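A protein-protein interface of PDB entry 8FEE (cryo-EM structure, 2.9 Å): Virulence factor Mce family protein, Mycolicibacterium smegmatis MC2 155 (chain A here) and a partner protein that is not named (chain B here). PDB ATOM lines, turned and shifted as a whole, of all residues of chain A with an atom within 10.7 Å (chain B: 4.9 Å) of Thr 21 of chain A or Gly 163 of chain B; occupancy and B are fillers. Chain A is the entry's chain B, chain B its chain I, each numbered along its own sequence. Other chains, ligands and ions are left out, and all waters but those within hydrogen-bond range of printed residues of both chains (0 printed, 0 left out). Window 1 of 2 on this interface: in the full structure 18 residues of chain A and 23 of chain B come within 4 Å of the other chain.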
ATOM      1  N   PHE A  13      12.532  25.107 -23.298  1.00  0.00           N
ATOM      2  CA  PHE A  13      12.129  23.937 -22.523  1.00  0.00           C
ATOM      3  C   PHE A  13      13.257  23.458 -21.617  1.00  0.00           C
ATOM      4  O   PHE A  13      13.026  23.122 -20.447  1.00  0.00           O
ATOM      5  CB  PHE A  13      11.678  22.815 -23.456  1.00  0.00           C
ATOM      6  CG  PHE A  13      10.196  22.580 -23.446  1.00  0.00           C
ATOM      7  CD1 PHE A  13       9.365  23.280 -24.304  1.00  0.00           C
ATOM      8  CD2 PHE A  13       9.635  21.656 -22.581  1.00  0.00           C
ATOM      9  CE1 PHE A  13       8.000  23.065 -24.297  1.00  0.00           C
ATOM     10  CE2 PHE A  13       8.271  21.437 -22.570  1.00  0.00           C
ATOM     11  CZ  PHE A  13       7.452  22.142 -23.430  1.00  0.00           C
ATOM     12  N   SER A  14      14.486  23.426 -22.138  1.00  0.00           N
ATOM     13  CA  SER A  14      15.624  23.012 -21.331  1.00  0.00           C
ATOM     14  C   SER A  14      15.890  24.001 -20.208  1.00  0.00           C
ATOM     15  O   SER A  14      16.228  23.596 -19.095  1.00  0.00           O
ATOM     16  CB  SER A  14      16.860  22.851 -22.215  1.00  0.00           C
ATOM     17  OG  SER A  14      16.713  21.745 -23.086  1.00  0.00           O
ATOM     18  N   LEU A  15      15.732  25.301 -20.474  1.00  0.00           N
ATOM     19  CA  LEU A  15      15.911  26.301 -19.429  1.00  0.00           C
ATOM     20  C   LEU A  15      14.924  26.082 -18.292  1.00  0.00           C
ATOM     21  O   LEU A  15      15.302  26.086 -17.118  1.00  0.00           O
ATOM     22  CB  LEU A  15      15.760  27.704 -20.016  1.00  0.00           C
ATOM     23  CG  LEU A  15      16.017  28.871 -19.062  1.00  0.00           C
ATOM     24  CD1 LEU A  15      17.477  28.903 -18.645  1.00  0.00           C
ATOM     25  CD2 LEU A  15      15.608  30.187 -19.703  1.00  0.00           C
ATOM     26  N   VAL A  16      13.652  25.855 -18.629  1.00  0.00           N
ATOM     27  CA  VAL A  16      12.636  25.661 -17.597  1.00  0.00           C
ATOM     28  C   VAL A  16      12.899  24.380 -16.807  1.00  0.00           C
ATOM     29  O   VAL A  16      12.828  24.368 -15.570  1.00  0.00           O
ATOM     30  CB  VAL A  16      11.229  25.662 -18.220  1.00  0.00           C
ATOM     31  CG1 VAL A  16      10.182  25.343 -17.168  1.00  0.00           C
ATOM     32  CG2 VAL A  16      10.937  27.008 -18.860  1.00  0.00           C
ATOM     33  N   LEU A  17      13.209  23.281 -17.501  1.00  0.00           N
ATOM     34  CA  LEU A  17      13.401  22.021 -16.785  1.00  0.00           C
ATOM     35  C   LEU A  17      14.688  22.016 -15.961  1.00  0.00           C
ATOM     36  O   LEU A  17      14.717  21.439 -14.866  1.00  0.00           O
ATOM     37  CB  LEU A  17      13.359  20.850 -17.765  1.00  0.00           C
ATOM     38  CG  LEU A  17      11.967  20.652 -18.382  1.00  0.00           C
ATOM     39  CD1 LEU A  17      11.853  19.339 -19.140  1.00  0.00           C
ATOM     40  CD2 LEU A  17      10.875  20.756 -17.327  1.00  0.00           C
ATOM     41  N   LEU A  18      15.749  22.672 -16.439  1.00  0.00           N
ATOM     42  CA  LEU A  18      16.954  22.798 -15.628  1.00  0.00           C
ATOM     43  C   LEU A  18      16.736  23.745 -14.457  1.00  0.00           C
ATOM     44  O   LEU A  18      17.344  23.563 -13.398  1.00  0.00           O
ATOM     45  CB  LEU A  18      18.131  23.270 -16.483  1.00  0.00           C
ATOM     46  CG  LEU A  18      18.645  22.306 -17.556  1.00  0.00           C
ATOM     47  CD1 LEU A  18      19.887  22.863 -18.233  1.00  0.00           C
ATOM     48  CD2 LEU A  18      18.919  20.936 -16.970  1.00  0.00           C
ATOM     49  N   THR A  19      15.871  24.749 -14.623  1.00  0.00           N
ATOM     50  CA  THR A  19      15.477  25.580 -13.492  1.00  0.00           C
ATOM     51  C   THR A  19      14.762  24.752 -12.434  1.00  0.00           C
ATOM     52  O   THR A  19      15.016  24.912 -11.235  1.00  0.00           O
ATOM     53  CB  THR A  19      14.592  26.731 -13.977  1.00  0.00           C
ATOM     54  OG1 THR A  19      15.398  27.693 -14.668  1.00  0.00           O
ATOM     55  CG2 THR A  19      13.893  27.416 -12.812  1.00  0.00           C
ATOM     56  N   PHE A  20      13.876  23.848 -12.858  1.00  0.00           N
ATOM     57  CA  PHE A  20      13.232  22.947 -11.902  1.00  0.00           C
ATOM     58  C   PHE A  20      14.247  22.040 -11.210  1.00  0.00           C
ATOM     59  O   PHE A  20      14.164  21.819  -9.995  1.00  0.00           O
ATOM     60  CB  PHE A  20      12.160  22.111 -12.600  1.00  0.00           C
ATOM     61  CG  PHE A  20      10.867  22.841 -12.819  1.00  0.00           C
ATOM     62  CD1 PHE A  20      10.558  23.966 -12.072  1.00  0.00           C
ATOM     63  CD2 PHE A  20       9.958  22.399 -13.764  1.00  0.00           C
ATOM     64  CE1 PHE A  20       9.369  24.638 -12.267  1.00  0.00           C
ATOM     65  CE2 PHE A  20       8.767  23.068 -13.965  1.00  0.00           C
ATOM     66  CZ  PHE A  20       8.472  24.189 -13.215  1.00  0.00           C
ATOM     67  N   THR A  21      15.205  21.496 -11.965  1.00  0.00           N
ATOM     68  CA  THR A  21      16.216  20.624 -11.363  1.00  0.00           C
ATOM     69  C   THR A  21      17.079  21.382 -10.356  1.00  0.00           C
ATOM     70  O   THR A  21      17.374  20.880  -9.260  1.00  0.00           O
ATOM     71  CB  THR A  21      17.086  19.999 -12.456  1.00  0.00           C
ATOM     72  OG1 THR A  21      16.269  19.197 -13.318  1.00  0.00           O
ATOM     73  CG2 THR A  21      18.168  19.123 -11.846  1.00  0.00           C
ATOM     74  N   ALA A  22      17.447  22.622 -10.685  1.00  0.00           N
ATOM     75  CA  ALA A  22      18.230  23.423  -9.756  1.00  0.00           C
ATOM     76  C   ALA A  22      17.405  23.826  -8.547  1.00  0.00           C
ATOM     77  O   ALA A  22      17.949  23.948  -7.446  1.00  0.00           O
ATOM     78  CB  ALA A  22      18.784  24.661 -10.461  1.00  0.00           C
ATOM     79  N   LEU A  23      16.105  24.064  -8.730  1.00  0.00           N
ATOM     80  CA  LEU A  23      15.243  24.329  -7.585  1.00  0.00           C
ATOM     81  C   LEU A  23      15.180  23.118  -6.665  1.00  0.00           C
ATOM     82  O   LEU A  23      15.156  23.262  -5.440  1.00  0.00           O
ATOM     83  CB  LEU A  23      13.845  24.716  -8.067  1.00  0.00           C
ATOM     84  CG  LEU A  23      12.761  24.877  -7.003  1.00  0.00           C
ATOM     85  CD1 LEU A  23      13.096  26.028  -6.071  1.00  0.00           C
ATOM     86  CD2 LEU A  23      11.407  25.087  -7.656  1.00  0.00           C
ATOM     87  N   ILE A  24      15.157  21.913  -7.243  1.00  0.00           N
ATOM     88  CA  ILE A  24      15.212  20.695  -6.434  1.00  0.00           C
ATOM     89  C   ILE A  24      16.499  20.654  -5.623  1.00  0.00           C
ATOM     90  O   ILE A  24      16.488  20.345  -4.422  1.00  0.00           O
ATOM     91  CB  ILE A  24      15.076  19.446  -7.324  1.00  0.00           C
ATOM     92  CG1 ILE A  24      13.687  19.376  -7.951  1.00  0.00           C
ATOM     93  CG2 ILE A  24      15.355  18.183  -6.525  1.00  0.00           C
ATOM     94  CD1 ILE A  24      13.512  18.196  -8.872  1.00  0.00           C
ATOM     95  N   PHE A  25      17.627  20.978  -6.264  1.00  0.00           N
ATOM     96  CA  PHE A  25      18.902  20.975  -5.547  1.00  0.00           C
ATOM     97  C   PHE A  25      18.930  22.027  -4.444  1.00  0.00           C
ATOM     98  O   PHE A  25      19.428  21.767  -3.344  1.00  0.00           O
ATOM     99  CB  PHE A  25      20.066  21.186  -6.515  1.00  0.00           C
ATOM    100  CG  PHE A  25      20.519  19.932  -7.207  1.00  0.00           C
ATOM    101  CD1 PHE A  25      21.365  19.043  -6.567  1.00  0.00           C
ATOM    102  CD2 PHE A  25      20.112  19.647  -8.498  1.00  0.00           C
ATOM    103  CE1 PHE A  25      21.789  17.890  -7.197  1.00  0.00           C
ATOM    104  CE2 PHE A  25      20.533  18.495  -9.133  1.00  0.00           C
ATOM    105  CZ  PHE A  25      21.373  17.616  -8.481  1.00  0.00           C
ATOM    106  N   VAL A  26      18.403  23.221  -4.719  1.00  0.00           N
ATOM    107  CA  VAL A  26      18.375  24.285  -3.718  1.00  0.00           C
ATOM    108  C   VAL A  26      17.496  23.890  -2.537  1.00  0.00           C
ATOM    109  O   VAL A  26      17.849  24.122  -1.375  1.00  0.00           O
ATOM    110  CB  VAL A  26      17.910  25.606  -4.362  1.00  0.00           C
ATOM    111  CG1 VAL A  26      17.523  26.621  -3.303  1.00  0.00           C
ATOM    112  CG2 VAL A  26      19.001  26.165  -5.256  1.00  0.00           C
ATOM    113  N   VAL A  27      16.344  23.273  -2.814  1.00  0.00           N
ATOM    114  CA  VAL A  27      15.412  22.923  -1.747  1.00  0.00           C
ATOM    115  C   VAL A  27      15.974  21.802  -0.882  1.00  0.00           C
ATOM    116  O   VAL A  27      15.920  21.871   0.352  1.00  0.00           O
ATOM    117  CB  VAL A  27      14.039  22.555  -2.340  1.00  0.00           C
ATOM    118  CG1 VAL A  27      13.179  21.853  -1.306  1.00  0.00           C
ATOM    119  CG2 VAL A  27      13.335  23.803  -2.836  1.00  0.00           C
ATOM    120  N   PHE A  28      16.536  20.764  -1.498  1.00  0.00           N
ATOM    121  CA  PHE A  28      16.975  19.598  -0.746  1.00  0.00           C
ATOM    122  C   PHE A  28      18.458  19.630  -0.401  1.00  0.00           C
ATOM    123  O   PHE A  28      18.983  18.640   0.118  1.00  0.00           O
ATOM    124  CB  PHE A  28      16.634  18.320  -1.511  1.00  0.00           C
ATOM    125  CG  PHE A  28      15.165  18.035  -1.568  1.00  0.00           C
ATOM    126  CD1 PHE A  28      14.538  17.376  -0.527  1.00  0.00           C
ATOM    127  CD2 PHE A  28      14.410  18.431  -2.655  1.00  0.00           C
ATOM    128  CE1 PHE A  28      13.188  17.112  -0.570  1.00  0.00           C
ATOM    129  CE2 PHE A  28      13.056  18.170  -2.704  1.00  0.00           C
ATOM    130  CZ  PHE A  28      12.446  17.510  -1.659  1.00  0.00           C
ATOM    131  N   GLY A  29      19.143  20.736  -0.671  1.00  0.00           N
ATOM    132  CA  GLY A  29      20.535  20.860  -0.289  1.00  0.00           C
ATOM    133  C   GLY A  29      20.765  21.970   0.713  1.00  0.00           C
ATOM    134  O   GLY A  29      21.899  22.195   1.149  1.00  0.00           O
ATOM    135  N   ILE A  31      20.583  25.302   0.432  1.00  0.00           N
ATOM    136  CA  ILE A  31      21.471  26.321  -0.112  1.00  0.00           C
ATOM    137  C   ILE A  31      20.943  27.695   0.277  1.00  0.00           C
ATOM    138  O   ILE A  31      19.760  27.995   0.075  1.00  0.00           O
ATOM    139  CB  ILE A  31      21.588  26.189  -1.639  1.00  0.00           C
ATOM    140  CG1 ILE A  31      21.987  24.764  -2.025  1.00  0.00           C
ATOM    141  CG2 ILE A  31      22.588  27.193  -2.188  1.00  0.00           C
ATOM    142  CD1 ILE A  31      23.273  24.296  -1.393  1.00  0.00           C
ATOM    143  N   PHE B 159      17.336  13.295 -18.131  1.00  0.00           N
ATOM    144  CA  PHE B 159      17.707  14.145 -17.000  1.00  0.00           C
ATOM    145  C   PHE B 159      16.636  15.201 -16.729  1.00  0.00           C
ATOM    146  O   PHE B 159      16.127  15.329 -15.599  1.00  0.00           O
ATOM    147  CB  PHE B 159      19.064  14.790 -17.296  1.00  0.00           C
ATOM    148  CG  PHE B 159      19.553  15.724 -16.230  1.00  0.00           C
ATOM    149  CD1 PHE B 159      20.248  15.243 -15.136  1.00  0.00           C
ATOM    150  CD2 PHE B 159      19.358  17.090 -16.344  1.00  0.00           C
ATOM    151  CE1 PHE B 159      20.711  16.103 -14.162  1.00  0.00           C
ATOM    152  CE2 PHE B 159      19.821  17.952 -15.371  1.00  0.00           C
ATOM    153  CZ  PHE B 159      20.498  17.458 -14.280  1.00  0.00           C
ATOM    154  N   MET B 160      16.267  15.957 -17.769  1.00  0.00           N
ATOM    155  CA  MET B 160      15.287  17.026 -17.596  1.00  0.00           C
ATOM    156  C   MET B 160      13.928  16.481 -17.166  1.00  0.00           C
ATOM    157  O   MET B 160      13.262  17.062 -16.295  1.00  0.00           O
ATOM    158  CB  MET B 160      15.170  17.826 -18.890  1.00  0.00           C
ATOM    159  CG  MET B 160      16.326  18.779 -19.120  1.00  0.00           C
ATOM    160  SD  MET B 160      16.465  19.308 -20.835  1.00  0.00           S
ATOM    161  CE  MET B 160      14.745  19.457 -21.292  1.00  0.00           C
ATOM    162  N   LEU B 161      13.499  15.367 -17.764  1.00  0.00           N
ATOM    163  CA  LEU B 161      12.200  14.797 -17.424  1.00  0.00           C
ATOM    164  C   LEU B 161      12.182  14.265 -16.000  1.00  0.00           C
ATOM    165  O   LEU B 161      11.158  14.359 -15.322  1.00  0.00           O
ATOM    166  CB  LEU B 161      11.821  13.697 -18.415  1.00  0.00           C
ATOM    167  CG  LEU B 161      11.491  14.135 -19.842  1.00  0.00           C
ATOM    168  CD1 LEU B 161      10.866  12.985 -20.610  1.00  0.00           C
ATOM    169  CD2 LEU B 161      10.578  15.350 -19.843  1.00  0.00           C
ATOM    170  N   ASN B 162      13.293  13.692 -15.528  1.00  0.00           N
ATOM    171  CA  ASN B 162      13.353  13.258 -14.135  1.00  0.00           C
ATOM    172  C   ASN B 162      13.201  14.439 -13.187  1.00  0.00           C
ATOM    173  O   ASN B 162      12.457  14.361 -12.195  1.00  0.00           O
ATOM    174  CB  ASN B 162      14.666  12.529 -13.870  1.00  0.00           C
ATOM    175  CG  ASN B 162      14.766  12.011 -12.452  1.00  0.00           C
ATOM    176  OD1 ASN B 162      13.793  11.510 -11.892  1.00  0.00           O
ATOM    177  ND2 ASN B 162      15.947  12.133 -11.860  1.00  0.00           N
ATOM    178  N   GLY B 163      13.895  15.543 -13.477  1.00  0.00           N
ATOM    179  CA  GLY B 163      13.729  16.734 -12.653  1.00  0.00           C
ATOM    180  C   GLY B 163      12.288  17.213 -12.623  1.00  0.00           C
ATOM    181  O   GLY B 163      11.729  17.508 -11.555  1.00  0.00           O
ATOM    182  N   ALA B 164      11.663  17.281 -13.803  1.00  0.00           N
ATOM    183  CA  ALA B 164      10.279  17.737 -13.888  1.00  0.00           C
ATOM    184  C   ALA B 164       9.340  16.799 -13.142  1.00  0.00           C
ATOM    185  O   ALA B 164       8.400  17.253 -12.478  1.00  0.00           O
ATOM    186  CB  ALA B 164       9.856  17.861 -15.351  1.00  0.00           C
ATOM    187  N   VAL B 165       9.571  15.486 -13.249  1.00  0.00           N
ATOM    188  CA  VAL B 165       8.727  14.512 -12.563  1.00  0.00           C
ATOM    189  C   VAL B 165       8.791  14.729 -11.062  1.00  0.00           C
ATOM    190  O   VAL B 165       7.761  14.756 -10.381  1.00  0.00           O
ATOM    191  CB  VAL B 165       9.135  13.076 -12.933  1.00  0.00           C
ATOM    192  CG1 VAL B 165       8.534  12.090 -11.951  1.00  0.00           C
ATOM    193  CG2 VAL B 165       8.662  12.741 -14.311  1.00  0.00           C
ATOM    194  N   ILE B 166      10.003  14.885 -10.522  1.00  0.00           N
ATOM    195  CA  ILE B 166      10.134  15.053  -9.076  1.00  0.00           C
ATOM    196  C   ILE B 166       9.420  16.322  -8.621  1.00  0.00           C
ATOM    197  O   ILE B 166       8.647  16.306  -7.650  1.00  0.00           O
ATOM    198  CB  ILE B 166      11.616  15.052  -8.660  1.00  0.00           C
ATOM    199  CG1 ILE B 166      12.275  13.728  -9.042  1.00  0.00           C
ATOM    200  CG2 ILE B 166      11.746  15.294  -7.166  1.00  0.00           C
ATOM    201  CD1 ILE B 166      13.715  13.615  -8.603  1.00  0.00           C
ATOM    202  N   THR B 167       9.648  17.436  -9.330  1.00  0.00           N
ATOM    203  CA  THR B 167       9.034  18.701  -8.919  1.00  0.00           C
ATOM    204  C   THR B 167       7.509  18.632  -8.980  1.00  0.00           C
ATOM    205  O   THR B 167       6.814  19.007  -8.022  1.00  0.00           O
ATOM    206  CB  THR B 167       9.547  19.843  -9.797  1.00  0.00           C
ATOM    207  OG1 THR B 167      10.929  20.086  -9.511  1.00  0.00           O
ATOM    208  CG2 THR B 167       8.756  21.114  -9.537  1.00  0.00           C
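The backbone carbonyl oxygen (O) of Leu 17 of chain A sits at hydrogen-bond distance from the side-chain hydroxyl (OG1) of Thr 21 of chain A (3.1 Å).
The backbone carbonyl oxygen of Gly 163 of chain B lies within hydrogen-bond range of the side-chain hydroxyl of Thr 167 of chain B (3.4 Å).
Of the 18 printed residues of chain A, 6 touch a printed residue of chain B.
Printed residues of chain A that touch a printed residue of chain B: Ser 14, Leu 17, Leu 18, Phe 20, Thr 21 and Ile 24.
Along chain A the printed residues that touch a printed residue of chain B span positions 14 to 24.
Of the printed residues of chain B, Ser 14 of chain A touches Met 160.
Printed residues of chain B within 4 Å of Leu 17 of chain A: Met 160 (3.6 Å) and Ala 164 (3.7 Å).
Of the printed residues of chain B, Leu 18 of chain A touches Phe 159 (3.5 Å) and Met 160 (3.9998 Å).
Printed residues of chain B within 4 Å of Phe 20 of chain A: Thr 167.
Of chain B, only Phe 159 and Gly 163 come within 4 Å of Thr 21 of chain A.
Ala 22 of chain A touches none of the printed residues of chain B.
Phe 159 of chain B touches just these residues of chain A: Leu 18 and Thr 21.
Printed residues of chain A within 4 Å of Met 160 of chain B: Ser 14 (3.3 Å), Leu 17 (3.6 Å) and Leu 18 (3.9998 Å).
Leu 161 of chain B touches none of the printed residues of chain A.
No residue of chain A comes within 4 Å of Asn 162 of chain B.
Of chain A, only Thr 21 (3.6 Å) and Ile 24 (3.3 Å) come within 4 Å of Gly 163 of chain B.
Val 165 of chain B touches none of the printed residues of chain A.
Ile 166 of chain B touches just one residue of chain A: Ile 24 (3.7 Å).
Thr 167 of chain B touches just these residues of chain A: Phe 20 (3.7 Å) and Ile 24 (3.2 Å).
The nearest residue of chain B that does not touch Thr 21 of chain A is Met 160 of chain B (4.7 Å).
The nearest residue of chain A that does not touch Gly 163 of chain B is Phe 20 of chain A (4.7 Å).
The nearest printed residue of chain A that does not touch Met 160 of chain B is Phe 13 of chain A (4.1 Å).
OG of Ser 14 of chain A sits at hydrogen-bond distance from SD of Met 160 of chain B.
CD1 of Leu 17 of chain A touches CE of Met 160 of chain B, 3.6 Å away.
Leu 17 of chain A touches Ala 164 of chain B (CD2 to CB, 3.7 Å).
CD2 of Leu 18 of chain A touches CE2 of Phe 159 of chain B, 3.5 Å away.
Leu 18 of chain A touches Met 160 of chain B.
Phe 20 of chain A touches Thr 167 of chain B.
Thr 21 of chain A touches Phe 159 of chain B (CG2 to CZ, 3.8 Å).
Gly 163 of chain B touches Thr 21 of chain A (CA to OG1, 3.6 Å).
Ile 24 of chain A touches Gly 163 of chain B.
Ile 24 of chain A touches Ile 166 of chain B (CD1 to CB, 3.7 Å).
Thr 167 of chain B touches Ile 24 of chain A.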
